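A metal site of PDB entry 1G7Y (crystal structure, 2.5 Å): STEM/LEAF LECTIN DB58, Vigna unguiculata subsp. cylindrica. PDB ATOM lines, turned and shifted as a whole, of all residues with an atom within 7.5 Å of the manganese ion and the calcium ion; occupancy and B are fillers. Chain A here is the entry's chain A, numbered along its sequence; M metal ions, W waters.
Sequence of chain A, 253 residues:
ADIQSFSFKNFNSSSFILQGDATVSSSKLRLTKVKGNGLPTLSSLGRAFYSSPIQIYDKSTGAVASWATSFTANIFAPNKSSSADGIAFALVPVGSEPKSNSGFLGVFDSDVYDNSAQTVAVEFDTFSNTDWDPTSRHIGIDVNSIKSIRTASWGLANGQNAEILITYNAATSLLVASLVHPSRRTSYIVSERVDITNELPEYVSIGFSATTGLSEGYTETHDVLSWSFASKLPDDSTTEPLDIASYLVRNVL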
ATOM      1  N   ASP A  85      16.949  -5.632   5.886  1.00  0.00           N
ATOM      2  CA  ASP A  85      17.717  -6.582   5.106  1.00  0.00           C
ATOM      3  C   ASP A  85      17.686  -6.193   3.619  1.00  0.00           C
ATOM      4  O   ASP A  85      18.609  -6.495   2.867  1.00  0.00           O
ATOM      5  CB  ASP A  85      17.107  -7.978   5.268  1.00  0.00           C
ATOM      6  CG  ASP A  85      17.743  -8.743   6.423  1.00  0.00           C
ATOM      7  OD1 ASP A  85      18.940  -9.067   6.328  1.00  0.00           O
ATOM      8  OD2 ASP A  85      17.042  -9.002   7.418  1.00  0.00           O
ATOM      9  N   GLY A  86      16.629  -5.509   3.208  1.00  0.00           N
ATOM     10  CA  GLY A  86      16.549  -5.096   1.810  1.00  0.00           C
ATOM     11  C   GLY A  86      15.194  -5.296   1.166  1.00  0.00           C
ATOM     12  O   GLY A  86      14.257  -5.792   1.790  1.00  0.00           O
ATOM     13  N   SER A 102      14.131 -12.276   6.902  1.00  0.00           N
ATOM     14  CA  SER A 102      15.429 -11.650   7.098  1.00  0.00           C
ATOM     15  C   SER A 102      16.318 -11.695   5.847  1.00  0.00           C
ATOM     16  O   SER A 102      15.943 -11.185   4.795  1.00  0.00           O
ATOM     17  CB  SER A 102      16.136 -12.300   8.288  1.00  0.00           C
ATOM     18  OG  SER A 102      17.297 -11.568   8.644  1.00  0.00           O
ATOM     19  N   GLY A 103      17.493 -12.301   5.977  1.00  0.00           N
ATOM     20  CA  GLY A 103      18.430 -12.386   4.864  1.00  0.00           C
ATOM     21  C   GLY A 103      17.917 -12.998   3.575  1.00  0.00           C
ATOM     22  O   GLY A 103      18.506 -12.777   2.514  1.00  0.00           O
ATOM     23  N   PHE A 104      16.828 -13.762   3.631  1.00  0.00           N
ATOM     24  CA  PHE A 104      16.288 -14.377   2.429  1.00  0.00           C
ATOM     25  C   PHE A 104      15.269 -13.481   1.719  1.00  0.00           C
ATOM     26  O   PHE A 104      14.686 -13.871   0.697  1.00  0.00           O
ATOM     27  CB  PHE A 104      15.691 -15.749   2.761  1.00  0.00           C
ATOM     28  CG  PHE A 104      16.697 -16.747   3.227  1.00  0.00           C
ATOM     29  CD1 PHE A 104      16.988 -16.885   4.581  1.00  0.00           C
ATOM     30  CD2 PHE A 104      17.412 -17.513   2.315  1.00  0.00           C
ATOM     31  CE1 PHE A 104      17.964 -17.782   5.017  1.00  0.00           C
ATOM     32  CE2 PHE A 104      18.384 -18.416   2.744  1.00  0.00           C
ATOM     33  CZ  PHE A 104      18.663 -18.555   4.091  1.00  0.00           C
ATOM     34  N   LEU A 105      15.047 -12.294   2.263  1.00  0.00           N
ATOM     35  CA  LEU A 105      14.140 -11.304   1.685  1.00  0.00           C
ATOM     36  C   LEU A 105      12.709 -11.777   1.382  1.00  0.00           C
ATOM     37  O   LEU A 105      11.981 -11.104   0.661  1.00  0.00           O
ATOM     38  CB  LEU A 105      14.774 -10.733   0.414  1.00  0.00           C
ATOM     39  CG  LEU A 105      16.198 -10.209   0.592  1.00  0.00           C
ATOM     40  CD1 LEU A 105      16.726  -9.663  -0.731  1.00  0.00           C
ATOM     41  CD2 LEU A 105      16.213  -9.119   1.650  1.00  0.00           C
ATOM     42  N   GLU A 123      17.690  -7.907  -6.280  1.00  0.00           N
ATOM     43  CA  GLU A 123      17.730  -7.448  -4.905  1.00  0.00           C
ATOM     44  C   GLU A 123      18.537  -6.192  -4.666  1.00  0.00           C
ATOM     45  O   GLU A 123      19.482  -5.866  -5.389  1.00  0.00           O
ATOM     46  CB  GLU A 123      18.283  -8.549  -3.998  1.00  0.00           C
ATOM     47  CG  GLU A 123      19.672  -9.028  -4.379  1.00  0.00           C
ATOM     48  CD  GLU A 123      20.313  -9.905  -3.328  1.00  0.00           C
ATOM     49  OE1 GLU A 123      19.731 -10.953  -2.984  1.00  0.00           O
ATOM     50  OE2 GLU A 123      21.410  -9.545  -2.847  1.00  0.00           O
ATOM     51  N   PHE A 124      18.127  -5.483  -3.631  1.00  0.00           N
ATOM     52  CA  PHE A 124      18.785  -4.266  -3.187  1.00  0.00           C
ATOM     53  C   PHE A 124      19.040  -4.608  -1.725  1.00  0.00           C
ATOM     54  O   PHE A 124      18.230  -4.324  -0.832  1.00  0.00           O
ATOM     55  CB  PHE A 124      17.841  -3.087  -3.416  1.00  0.00           C
ATOM     56  CG  PHE A 124      17.479  -2.921  -4.856  1.00  0.00           C
ATOM     57  CD1 PHE A 124      18.331  -2.240  -5.738  1.00  0.00           C
ATOM     58  CD2 PHE A 124      16.376  -3.578  -5.390  1.00  0.00           C
ATOM     59  CE1 PHE A 124      18.088  -2.228  -7.106  1.00  0.00           C
ATOM     60  CE2 PHE A 124      16.118  -3.575  -6.757  1.00  0.00           C
ATOM     61  CZ  PHE A 124      16.983  -2.892  -7.619  1.00  0.00           C
ATOM     62  N   ASP A 125      20.171  -5.288  -1.538  1.00  0.00           N
ATOM     63  CA  ASP A 125      20.661  -5.823  -0.282  1.00  0.00           C
ATOM     64  C   ASP A 125      21.409  -4.803   0.583  1.00  0.00           C
ATOM     65  O   ASP A 125      22.508  -4.382   0.237  1.00  0.00           O
ATOM     66  CB  ASP A 125      21.593  -6.985  -0.611  1.00  0.00           C
ATOM     67  CG  ASP A 125      21.621  -8.040   0.448  1.00  0.00           C
ATOM     68  OD1 ASP A 125      21.534  -7.698   1.649  1.00  0.00           O
ATOM     69  OD2 ASP A 125      21.744  -9.226   0.080  1.00  0.00           O
ATOM     70  N   THR A 126      20.826  -4.460   1.721  1.00  0.00           N
ATOM     71  CA  THR A 126      21.432  -3.488   2.628  1.00  0.00           C
ATOM     72  C   THR A 126      22.236  -4.115   3.764  1.00  0.00           C
ATOM     73  O   THR A 126      22.926  -3.397   4.494  1.00  0.00           O
ATOM     74  CB  THR A 126      20.378  -2.592   3.245  1.00  0.00           C
ATOM     75  OG1 THR A 126      19.422  -3.409   3.930  1.00  0.00           O
ATOM     76  CG2 THR A 126      19.662  -1.772   2.168  1.00  0.00           C
ATOM     77  N   PHE A 127      22.143  -5.435   3.927  1.00  0.00           N
ATOM     78  CA  PHE A 127      22.866  -6.124   4.988  1.00  0.00           C
ATOM     79  C   PHE A 127      23.669  -7.292   4.460  1.00  0.00           C
ATOM     80  O   PHE A 127      23.143  -8.186   3.799  1.00  0.00           O
ATOM     81  CB  PHE A 127      21.900  -6.593   6.069  1.00  0.00           C
ATOM     82  CG  PHE A 127      22.541  -7.446   7.114  1.00  0.00           C
ATOM     83  CD1 PHE A 127      22.548  -8.838   6.993  1.00  0.00           C
ATOM     84  CD2 PHE A 127      23.157  -6.868   8.226  1.00  0.00           C
ATOM     85  CE1 PHE A 127      23.143  -9.637   7.971  1.00  0.00           C
ATOM     86  CE2 PHE A 127      23.756  -7.661   9.212  1.00  0.00           C
ATOM     87  CZ  PHE A 127      23.751  -9.054   9.084  1.00  0.00           C
ATOM     88  N   SER A 128      24.956  -7.292   4.775  1.00  0.00           N
ATOM     89  CA  SER A 128      25.846  -8.337   4.297  1.00  0.00           C
ATOM     90  C   SER A 128      25.851  -9.647   5.093  1.00  0.00           C
ATOM     91  O   SER A 128      26.377  -9.702   6.202  1.00  0.00           O
ATOM     92  CB  SER A 128      27.269  -7.778   4.235  1.00  0.00           C
ATOM     93  OG  SER A 128      28.148  -8.714   3.640  1.00  0.00           O
ATOM     94  N   ASN A 129      25.325 -10.708   4.490  1.00  0.00           N
ATOM     95  CA  ASN A 129      25.294 -12.038   5.096  1.00  0.00           C
ATOM     96  C   ASN A 129      26.604 -12.724   4.720  1.00  0.00           C
ATOM     97  O   ASN A 129      26.748 -13.189   3.596  1.00  0.00           O
ATOM     98  CB  ASN A 129      24.132 -12.855   4.532  1.00  0.00           C
ATOM     99  CG  ASN A 129      22.776 -12.281   4.872  1.00  0.00           C
ATOM    100  OD1 ASN A 129      22.453 -11.140   4.520  1.00  0.00           O
ATOM    101  ND2 ASN A 129      21.959 -13.065   5.557  1.00  0.00           N
ATOM    102  N   THR A 130      27.552 -12.805   5.654  1.00  0.00           N
ATOM    103  CA  THR A 130      28.848 -13.413   5.331  1.00  0.00           C
ATOM    104  C   THR A 130      28.809 -14.761   4.619  1.00  0.00           C
ATOM    105  O   THR A 130      29.739 -15.098   3.880  1.00  0.00           O
ATOM    106  CB  THR A 130      29.747 -13.551   6.592  1.00  0.00           C
ATOM    107  OG1 THR A 130      29.013 -14.158   7.662  1.00  0.00           O
ATOM    108  CG2 THR A 130      30.262 -12.192   7.029  1.00  0.00           C
ATOM    109  N   TRP A 132      27.194 -15.695   2.070  1.00  0.00           N
ATOM    110  CA  TRP A 132      26.956 -15.685   0.646  1.00  0.00           C
ATOM    111  C   TRP A 132      27.018 -14.291   0.026  1.00  0.00           C
ATOM    112  O   TRP A 132      27.121 -14.168  -1.188  1.00  0.00           O
ATOM    113  CB  TRP A 132      25.592 -16.318   0.347  1.00  0.00           C
ATOM    114  CG  TRP A 132      24.386 -15.567   0.926  1.00  0.00           C
ATOM    115  CD1 TRP A 132      23.973 -14.294   0.591  1.00  0.00           C
ATOM    116  CD2 TRP A 132      23.461 -16.031   1.927  1.00  0.00           C
ATOM    117  NE1 TRP A 132      22.852 -13.958   1.313  1.00  0.00           N
ATOM    118  CE2 TRP A 132      22.510 -15.002   2.139  1.00  0.00           C
ATOM    119  CE3 TRP A 132      23.327 -17.225   2.650  1.00  0.00           C
ATOM    120  CZ2 TRP A 132      21.455 -15.125   3.053  1.00  0.00           C
ATOM    121  CZ3 TRP A 132      22.273 -17.349   3.564  1.00  0.00           C
ATOM    122  CH2 TRP A 132      21.351 -16.302   3.747  1.00  0.00           C
ATOM    123  N   ASP A 133      26.930 -13.259   0.847  1.00  0.00           N
ATOM    124  CA  ASP A 133      26.970 -11.902   0.327  1.00  0.00           C
ATOM    125  C   ASP A 133      28.348 -11.281   0.149  1.00  0.00           C
ATOM    126  O   ASP A 133      29.351 -11.774   0.676  1.00  0.00           O
ATOM    127  CB  ASP A 133      26.188 -10.930   1.222  1.00  0.00           C
ATOM    128  CG  ASP A 133      24.696 -10.994   0.994  1.00  0.00           C
ATOM    129  OD1 ASP A 133      24.271 -11.368  -0.122  1.00  0.00           O
ATOM    130  OD2 ASP A 133      23.951 -10.632   1.943  1.00  0.00           O
ATOM    131  N   PRO A 134      28.409 -10.201  -0.638  1.00  0.00           N
ATOM    132  CA  PRO A 134      29.668  -9.497  -0.870  1.00  0.00           C
ATOM    133  C   PRO A 134      29.826  -8.646   0.392  1.00  0.00           C
ATOM    134  O   PRO A 134      28.909  -8.568   1.206  1.00  0.00           O
ATOM    135  CB  PRO A 134      29.352  -8.638  -2.097  1.00  0.00           C
ATOM    136  CG  PRO A 134      28.315  -9.429  -2.802  1.00  0.00           C
ATOM    137  CD  PRO A 134      27.424  -9.864  -1.675  1.00  0.00           C
ATOM    138  N   SER A 136      29.970  -5.241   0.867  1.00  0.00           N
ATOM    139  CA  SER A 136      29.134  -4.063   1.035  1.00  0.00           C
ATOM    140  C   SER A 136      27.710  -4.222   0.545  1.00  0.00           C
ATOM    141  O   SER A 136      27.340  -5.274   0.025  1.00  0.00           O
ATOM    142  CB  SER A 136      29.786  -2.881   0.303  1.00  0.00           C
ATOM    143  OG  SER A 136      29.935  -3.182  -1.077  1.00  0.00           O
ATOM    144  N   ARG A 137      26.915  -3.167   0.728  1.00  0.00           N
ATOM    145  CA  ARG A 137      25.537  -3.168   0.262  1.00  0.00           C
ATOM    146  C   ARG A 137      25.648  -3.346  -1.247  1.00  0.00           C
ATOM    147  O   ARG A 137      26.594  -2.855  -1.858  1.00  0.00           O
ATOM    148  CB  ARG A 137      24.863  -1.850   0.624  1.00  0.00           C
ATOM    149  CG  ARG A 137      24.789  -1.619   2.125  1.00  0.00           C
ATOM    150  CD  ARG A 137      23.768  -0.548   2.477  1.00  0.00           C
ATOM    151  NE  ARG A 137      23.772  -0.261   3.905  1.00  0.00           N
ATOM    152  CZ  ARG A 137      24.742   0.407   4.525  1.00  0.00           C
ATOM    153  NH1 ARG A 137      25.779   0.868   3.836  1.00  0.00           N
ATOM    154  NH2 ARG A 137      24.671   0.629   5.834  1.00  0.00           N
ATOM    155  N   HIS A 138      24.686  -4.025  -1.846  1.00  0.00           N
ATOM    156  CA  HIS A 138      24.794  -4.290  -3.265  1.00  0.00           C
ATOM    157  C   HIS A 138      23.471  -4.529  -3.977  1.00  0.00           C
ATOM    158  O   HIS A 138      22.437  -4.748  -3.344  1.00  0.00           O
ATOM    159  CB  HIS A 138      25.637  -5.542  -3.444  1.00  0.00           C
ATOM    160  CG  HIS A 138      25.160  -6.701  -2.621  1.00  0.00           C
ATOM    161  ND1 HIS A 138      25.347  -6.779  -1.253  1.00  0.00           N
ATOM    162  CD2 HIS A 138      24.417  -7.790  -2.951  1.00  0.00           C
ATOM    163  CE1 HIS A 138      24.739  -7.854  -0.789  1.00  0.00           C
ATOM    164  NE2 HIS A 138      24.170  -8.489  -1.792  1.00  0.00           N
ATOM    165  N   ILE A 139      23.536  -4.489  -5.298  1.00  0.00           N
ATOM    166  CA  ILE A 139      22.399  -4.780  -6.157  1.00  0.00           C
ATOM    167  C   ILE A 139      22.774  -6.161  -6.667  1.00  0.00           C
ATOM    168  O   ILE A 139      23.938  -6.403  -6.984  1.00  0.00           O
ATOM    169  CB  ILE A 139      22.329  -3.852  -7.381  1.00  0.00           C
ATOM    170  CG1 ILE A 139      22.173  -2.405  -6.937  1.00  0.00           C
ATOM    171  CG2 ILE A 139      21.144  -4.261  -8.255  1.00  0.00           C
ATOM    172  CD1 ILE A 139      22.252  -1.434  -8.105  1.00  0.00           C
ATOM    173  N   GLY A 140      21.817  -7.067  -6.736  1.00  0.00           N
ATOM    174  CA  GLY A 140      22.152  -8.397  -7.214  1.00  0.00           C
ATOM    175  C   GLY A 140      21.054  -9.071  -8.004  1.00  0.00           C
ATOM    176  O   GLY A 140      19.873  -8.772  -7.840  1.00  0.00           O
ATOM    177  N   ASP A 142      19.266 -12.490  -8.548  1.00  0.00           N
ATOM    178  CA  ASP A 142      19.056 -13.780  -7.916  1.00  0.00           C
ATOM    179  C   ASP A 142      18.234 -14.723  -8.781  1.00  0.00           C
ATOM    180  O   ASP A 142      17.106 -14.415  -9.158  1.00  0.00           O
ATOM    181  CB  ASP A 142      18.337 -13.607  -6.578  1.00  0.00           C
ATOM    182  CG  ASP A 142      19.092 -12.701  -5.618  1.00  0.00           C
ATOM    183  OD1 ASP A 142      20.283 -12.405  -5.861  1.00  0.00           O
ATOM    184  OD2 ASP A 142      18.489 -12.292  -4.598  1.00  0.00           O
ATOM    185  N   ILE A 146      19.438 -17.302  -3.032  1.00  0.00           N
ATOM    186  CA  ILE A 146      19.721 -16.002  -2.470  1.00  0.00           C
ATOM    187  C   ILE A 146      21.159 -15.623  -2.795  1.00  0.00           C
ATOM    188  O   ILE A 146      21.543 -14.465  -2.627  1.00  0.00           O
ATOM    189  CB  ILE A 146      19.496 -15.989  -0.947  1.00  0.00           C
ATOM    190  CG1 ILE A 146      19.558 -14.539  -0.445  1.00  0.00           C
ATOM    191  CG2 ILE A 146      20.527 -16.859  -0.251  1.00  0.00           C
ATOM    192  CD1 ILE A 146      18.442 -13.667  -0.945  1.00  0.00           C
ATOM    193  N   LYS A 147      21.958 -16.584  -3.244  1.00  0.00           N
ATOM    194  CA  LYS A 147      23.351 -16.292  -3.597  1.00  0.00           C
ATOM    195  C   LYS A 147      23.373 -15.756  -5.025  1.00  0.00           C
ATOM    196  O   LYS A 147      23.410 -16.533  -5.969  1.00  0.00           O
ATOM    197  CB  LYS A 147      24.208 -17.577  -3.516  1.00  0.00           C
ATOM    198  CG  LYS A 147      25.737 -17.386  -3.626  1.00  0.00           C
ATOM    199  CD  LYS A 147      26.399 -18.738  -3.925  1.00  0.00           C
ATOM    200  CE  LYS A 147      27.684 -18.969  -3.157  1.00  0.00           C
ATOM    201  NZ  LYS A 147      28.795 -18.065  -3.557  1.00  0.00           N
ATOM    202  N   SER A 148      23.337 -14.428  -5.174  1.00  0.00           N
ATOM    203  CA  SER A 148      23.329 -13.767  -6.497  1.00  0.00           C
ATOM    204  C   SER A 148      24.331 -14.374  -7.476  1.00  0.00           C
ATOM    205  O   SER A 148      25.417 -14.813  -7.094  1.00  0.00           O
ATOM    206  CB  SER A 148      23.644 -12.267  -6.376  1.00  0.00           C
ATOM    207  OG  SER A 148      22.730 -11.576  -5.540  1.00  0.00           O
ATOM    208  N   THR A 151      26.682  -9.398  -8.788  1.00  0.00           N
ATOM    209  CA  THR A 151      26.319  -8.270  -7.940  1.00  0.00           C
ATOM    210  C   THR A 151      27.141  -7.049  -8.312  1.00  0.00           C
ATOM    211  O   THR A 151      28.076  -7.143  -9.092  1.00  0.00           O
ATOM    212  CB  THR A 151      26.582  -8.576  -6.456  1.00  0.00           C
ATOM    213  OG1 THR A 151      27.983  -8.782  -6.247  1.00  0.00           O
ATOM    214  CG2 THR A 151      25.835  -9.835  -6.033  1.00  0.00           C
HETATM  215 MN    MN M   1      22.881 -10.205  -1.410  1.00  0.00          MN
HETATM  216 CA    CA M   2      22.037  -9.808   2.586  1.00  0.00          CA
HETATM  217  O   HOH W   1      20.953 -11.664   1.718  1.00  0.00           O
HETATM  218  O   HOH W   2      21.603 -11.933  -1.094  1.00  0.00           O
HETATM  219  O   HOH W   3      20.228  -8.841   3.689  1.00  0.00           O
HETATM  220  O   HOH W   4      23.945 -11.361  -2.697  1.00  0.00           O
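The side-chain carboxylate of Glu 123 sits close to the side-chain carboxylate of Asp 142 (2.4 Å). N of Glu 123 is in hydrogen-bond range of O of Gly 140 (2.8 Å). The backbone carbonyl oxygen (O) of Ser 136 lies within hydrogen-bond range of a ring nitrogen (ND1) of His 138 (2.8 Å). The side-chain carboxylate (OD1) of Asp 133 lies close to the indole nitrogen (NE1) of Trp 132 (3.3 Å).
Within 4 Å of the manganese ion: Glu 123, Asp 125, Asp 133 and His 138. Along chain A the residues within 4 Å of the manganese ion span positions 123 to 138.
The nearest printed residue that does not touch the calcium ion is Trp 132 (4.4 Å).
Water W4 binds the manganese ion, at 2.0 Å. The manganese ion is bound by OD2 of Asp 125 (2.1 Å). The side-chain carboxylate (OE2) of Glu 123 binds the manganese ion. Water W2 is bound to the manganese ion (2.2 Å). A ring nitrogen (NE2) of His 138 binds the manganese ion (2.2 Å). OD1 of Asp 133 binds the manganese ion, 2.2 Å away. The manganese ion has six donor atoms within binding distance.
The calcium ion is bound by OD2 of Asp 133 (2.2 Å), O of Phe 127 (2.3 Å), water W1 (2.3 Å), water W3 (2.3 Å), OD1 of Asp 125 (2.4 Å), OD1 of Asn 129 (2.4 Å) and OD2 of Asp 125 (2.6 Å).
Water W2 lies within hydrogen-bond range of OE1 of Glu 123, O of Ile 146 and NE1 of Trp 132. Water W1 lies within hydrogen-bond range of the backbone carbonyl oxygen (O) of Gly 103 (2.8 Å) and the indole nitrogen (NE1) of Trp 132 (3.0 Å).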
